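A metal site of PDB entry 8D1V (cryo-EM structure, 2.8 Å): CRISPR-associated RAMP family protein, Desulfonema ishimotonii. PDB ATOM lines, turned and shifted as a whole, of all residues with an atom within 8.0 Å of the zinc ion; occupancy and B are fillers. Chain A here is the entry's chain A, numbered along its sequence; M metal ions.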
ATOM      1  N   ARG A 452       4.233   8.679   1.393  1.00  0.00           N
ATOM      2  CA  ARG A 452       4.815   8.927   2.702  1.00  0.00           C
ATOM      3  C   ARG A 452       5.334  10.349   2.819  1.00  0.00           C
ATOM      4  O   ARG A 452       5.174  11.008   3.857  1.00  0.00           O
ATOM      5  CB  ARG A 452       5.929   7.920   2.988  1.00  0.00           C
ATOM      6  CG  ARG A 452       6.792   8.289   4.175  1.00  0.00           C
ATOM      7  CD  ARG A 452       7.865   7.255   4.424  1.00  0.00           C
ATOM      8  NE  ARG A 452       7.311   5.907   4.487  1.00  0.00           N
ATOM      9  CZ  ARG A 452       6.623   5.422   5.509  1.00  0.00           C
ATOM     10  NH1 ARG A 452       6.353   6.158   6.572  1.00  0.00           N
ATOM     11  NH2 ARG A 452       6.187   4.170   5.461  1.00  0.00           N
ATOM     12  N   GLN A 456       3.593  13.384   5.274  1.00  0.00           N
ATOM     13  CA  GLN A 456       4.337  14.179   6.241  1.00  0.00           C
ATOM     14  C   GLN A 456       4.124  15.671   6.025  1.00  0.00           C
ATOM     15  O   GLN A 456       4.042  16.435   6.995  1.00  0.00           O
ATOM     16  CB  GLN A 456       5.826  13.830   6.162  1.00  0.00           C
ATOM     17  CG  GLN A 456       6.180  12.559   6.887  1.00  0.00           C
ATOM     18  CD  GLN A 456       7.437  11.919   6.347  1.00  0.00           C
ATOM     19  OE1 GLN A 456       8.482  11.945   6.981  1.00  0.00           O
ATOM     20  NE2 GLN A 456       7.334  11.328   5.163  1.00  0.00           N
ATOM     21  N   SER A 461       4.682  17.287  10.241  1.00  0.00           N
ATOM     22  CA  SER A 461       5.565  16.580  11.136  1.00  0.00           C
ATOM     23  C   SER A 461       6.317  15.508  10.367  1.00  0.00           C
ATOM     24  O   SER A 461       5.686  14.586   9.831  1.00  0.00           O
ATOM     25  CB  SER A 461       4.774  15.929  12.282  1.00  0.00           C
ATOM     26  OG  SER A 461       4.040  16.897  13.027  1.00  0.00           O
ATOM     27  N   PRO A 462       7.636  15.591  10.265  1.00  0.00           N
ATOM     28  CA  PRO A 462       8.397  14.498   9.666  1.00  0.00           C
ATOM     29  C   PRO A 462       8.375  13.270  10.560  1.00  0.00           C
ATOM     30  O   PRO A 462       8.034  13.323  11.739  1.00  0.00           O
ATOM     31  CB  PRO A 462       9.810  15.068   9.524  1.00  0.00           C
ATOM     32  CG  PRO A 462       9.668  16.555   9.732  1.00  0.00           C
ATOM     33  CD  PRO A 462       8.489  16.726  10.635  1.00  0.00           C
ATOM     34  N   CYS A 463       8.728  12.131   9.966  1.00  0.00           N
ATOM     35  CA  CYS A 463       8.872  10.877  10.678  1.00  0.00           C
ATOM     36  C   CYS A 463      10.358  10.585  10.836  1.00  0.00           C
ATOM     37  O   CYS A 463      11.081  10.417   9.848  1.00  0.00           O
ATOM     38  CB  CYS A 463       8.173   9.738   9.944  1.00  0.00           C
ATOM     39  SG  CYS A 463       8.482   8.131  10.700  1.00  0.00           S
ATOM     40  N   ASN A 464      10.821  10.543  12.079  1.00  0.00           N
ATOM     41  CA  ASN A 464      12.237  10.354  12.390  1.00  0.00           C
ATOM     42  C   ASN A 464      12.564   8.929  12.811  1.00  0.00           C
ATOM     43  O   ASN A 464      13.682   8.680  13.284  1.00  0.00           O
ATOM     44  CB  ASN A 464      12.676  11.353  13.457  1.00  0.00           C
ATOM     45  CG  ASN A 464      11.965  11.171  14.794  1.00  0.00           C
ATOM     46  OD1 ASN A 464      11.215  10.222  14.993  1.00  0.00           O
ATOM     47  ND2 ASN A 464      12.215  12.093  15.712  1.00  0.00           N
ATOM     48  N   ALA A 465      11.639   7.990  12.658  1.00  0.00           N
ATOM     49  CA  ALA A 465      11.892   6.611  13.041  1.00  0.00           C
ATOM     50  C   ALA A 465      12.965   5.988  12.159  1.00  0.00           C
ATOM     51  O   ALA A 465      13.034   6.244  10.944  1.00  0.00           O
ATOM     52  CB  ALA A 465      10.609   5.783  12.950  1.00  0.00           C
ATOM     53  N   GLU A 466      13.809   5.168  12.766  1.00  0.00           N
ATOM     54  CA  GLU A 466      14.864   4.477  12.050  1.00  0.00           C
ATOM     55  C   GLU A 466      14.409   3.073  11.664  1.00  0.00           C
ATOM     56  O   GLU A 466      13.377   2.575  12.108  1.00  0.00           O
ATOM     57  CB  GLU A 466      16.146   4.445  12.883  1.00  0.00           C
ATOM     58  CG  GLU A 466      16.054   3.592  14.141  1.00  0.00           C
ATOM     59  CD  GLU A 466      15.645   4.399  15.360  1.00  0.00           C
ATOM     60  OE1 GLU A 466      15.427   5.611  15.226  1.00  0.00           O
ATOM     61  OE2 GLU A 466      15.532   3.807  16.456  1.00  0.00           O
ATOM     62  N   PRO A 471       7.203  -1.154  15.106  1.00  0.00           N
ATOM     63  CA  PRO A 471       6.725  -0.193  14.101  1.00  0.00           C
ATOM     64  C   PRO A 471       6.483   1.192  14.691  1.00  0.00           C
ATOM     65  O   PRO A 471       5.954   1.332  15.795  1.00  0.00           O
ATOM     66  CB  PRO A 471       5.409  -0.817  13.601  1.00  0.00           C
ATOM     67  CG  PRO A 471       5.549  -2.256  13.906  1.00  0.00           C
ATOM     68  CD  PRO A 471       6.373  -2.365  15.143  1.00  0.00           C
ATOM     69  N   CYS A 472       6.870   2.211  13.931  1.00  0.00           N
ATOM     70  CA  CYS A 472       6.633   3.582  14.341  1.00  0.00           C
ATOM     71  C   CYS A 472       5.141   3.859  14.440  1.00  0.00           C
ATOM     72  O   CYS A 472       4.369   3.432  13.584  1.00  0.00           O
ATOM     73  CB  CYS A 472       7.291   4.549  13.351  1.00  0.00           C
ATOM     74  SG  CYS A 472       7.342   6.278  13.887  1.00  0.00           S
ATOM     75  N   MET A 473       4.743   4.562  15.488  1.00  0.00           N
ATOM     76  CA  MET A 473       3.329   4.807  15.771  1.00  0.00           C
ATOM     77  C   MET A 473       2.916   6.240  15.475  1.00  0.00           C
ATOM     78  O   MET A 473       1.895   6.715  15.974  1.00  0.00           O
ATOM     79  CB  MET A 473       3.016   4.441  17.222  1.00  0.00           C
ATOM     80  CG  MET A 473       3.348   3.017  17.596  1.00  0.00           C
ATOM     81  SD  MET A 473       2.416   1.779  16.668  1.00  0.00           S
ATOM     82  CE  MET A 473       0.756   2.424  16.842  1.00  0.00           C
ATOM     83  N   CYS A 474       3.682   6.951  14.655  1.00  0.00           N
ATOM     84  CA  CYS A 474       3.319   8.299  14.250  1.00  0.00           C
ATOM     85  C   CYS A 474       2.176   8.238  13.255  1.00  0.00           C
ATOM     86  O   CYS A 474       1.831   7.165  12.742  1.00  0.00           O
ATOM     87  CB  CYS A 474       4.515   9.044  13.643  1.00  0.00           C
ATOM     88  SG  CYS A 474       4.916   8.623  11.946  1.00  0.00           S
ATOM     89  N   LYS A 475       1.564   9.391  13.002  1.00  0.00           N
ATOM     90  CA  LYS A 475       0.375   9.437  12.167  1.00  0.00           C
ATOM     91  C   LYS A 475       0.683   8.972  10.742  1.00  0.00           C
ATOM     92  O   LYS A 475      -0.171   8.353  10.094  1.00  0.00           O
ATOM     93  CB  LYS A 475      -0.215  10.843  12.156  1.00  0.00           C
ATOM     94  CG  LYS A 475      -0.604  11.360  13.523  1.00  0.00           C
ATOM     95  CD  LYS A 475      -0.741  12.863  13.535  1.00  0.00           C
ATOM     96  CE  LYS A 475       0.603  13.544  13.270  1.00  0.00           C
ATOM     97  NZ  LYS A 475       0.489  15.021  13.305  1.00  0.00           N
ATOM     98  N   THR A 476       1.872   9.295  10.239  1.00  0.00           N
ATOM     99  CA  THR A 476       2.234   8.910   8.882  1.00  0.00           C
ATOM    100  C   THR A 476       2.455   7.413   8.774  1.00  0.00           C
ATOM    101  O   THR A 476       1.930   6.765   7.861  1.00  0.00           O
ATOM    102  CB  THR A 476       3.482   9.677   8.435  1.00  0.00           C
ATOM    103  OG1 THR A 476       3.153  11.058   8.271  1.00  0.00           O
ATOM    104  CG2 THR A 476       4.014   9.124   7.126  1.00  0.00           C
ATOM    105  N   CYS A 477       3.213   6.830   9.705  1.00  0.00           N
ATOM    106  CA  CYS A 477       3.460   5.387   9.668  1.00  0.00           C
ATOM    107  C   CYS A 477       2.183   4.588   9.857  1.00  0.00           C
ATOM    108  O   CYS A 477       2.037   3.531   9.247  1.00  0.00           O
ATOM    109  CB  CYS A 477       4.471   4.985  10.729  1.00  0.00           C
ATOM    110  SG  CYS A 477       6.165   5.425  10.350  1.00  0.00           S
ATOM    111  N   ARG A 478       1.273   5.050  10.708  1.00  0.00           N
ATOM    112  CA  ARG A 478       0.027   4.326  10.928  1.00  0.00           C
ATOM    113  C   ARG A 478      -0.802   4.249   9.657  1.00  0.00           C
ATOM    114  O   ARG A 478      -1.387   3.218   9.334  1.00  0.00           O
ATOM    115  CB  ARG A 478      -0.763   4.977  12.057  1.00  0.00           C
ATOM    116  CG  ARG A 478      -0.257   4.620  13.442  1.00  0.00           C
ATOM    117  CD  ARG A 478      -1.242   5.034  14.522  1.00  0.00           C
ATOM    118  NE  ARG A 478      -0.788   6.201  15.270  1.00  0.00           N
ATOM    119  CZ  ARG A 478      -1.316   7.410  15.165  1.00  0.00           C
ATOM    120  NH1 ARG A 478      -2.335   7.653  14.353  1.00  0.00           N
ATOM    121  NH2 ARG A 478      -0.819   8.404  15.900  1.00  0.00           N
ATOM    122  N   ARG A 481       0.862   1.846   7.003  1.00  0.00           N
ATOM    123  CA  ARG A 481       0.789   0.411   7.252  1.00  0.00           C
ATOM    124  C   ARG A 481      -0.524  -0.199   6.795  1.00  0.00           C
ATOM    125  O   ARG A 481      -0.635  -1.431   6.741  1.00  0.00           O
ATOM    126  CB  ARG A 481       0.999   0.131   8.740  1.00  0.00           C
ATOM    127  CG  ARG A 481       2.452   0.104   9.136  1.00  0.00           C
ATOM    128  CD  ARG A 481       2.645  -0.593  10.455  1.00  0.00           C
ATOM    129  NE  ARG A 481       1.862   0.038  11.501  1.00  0.00           N
ATOM    130  CZ  ARG A 481       2.294   1.030  12.265  1.00  0.00           C
ATOM    131  NH1 ARG A 481       3.523   1.507  12.137  1.00  0.00           N
ATOM    132  NH2 ARG A 481       1.483   1.549  13.184  1.00  0.00           N
HETATM  133 ZN    ZN M   1       6.706   7.140  11.812  1.00  0.00          ZN
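The side-chain amide oxygen of Gln 456 lies within hydrogen-bond range of the backbone NH of Cys 463 (3.0 Å). The backbone NH of Thr 476 sits close to the side-chain sulfur of Cys 474, 3.6 Å away. SG of Cys 463 lies close to N of Ala 465 (3.7 Å). O of Cys 472 sits at hydrogen-bond distance from NH1 of Arg 481 (2.6 Å).
Four residues have an atom within 4 Å of the zinc ion: Cys 463, Cys 472, Cys 474 and Cys 477.
The zinc ion is bound by SG of Cys 477 (2.3 Å), SG of Cys 463 (2.3 Å), SG of Cys 474 (2.3 Å) and SG of Cys 472 (2.3 Å).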
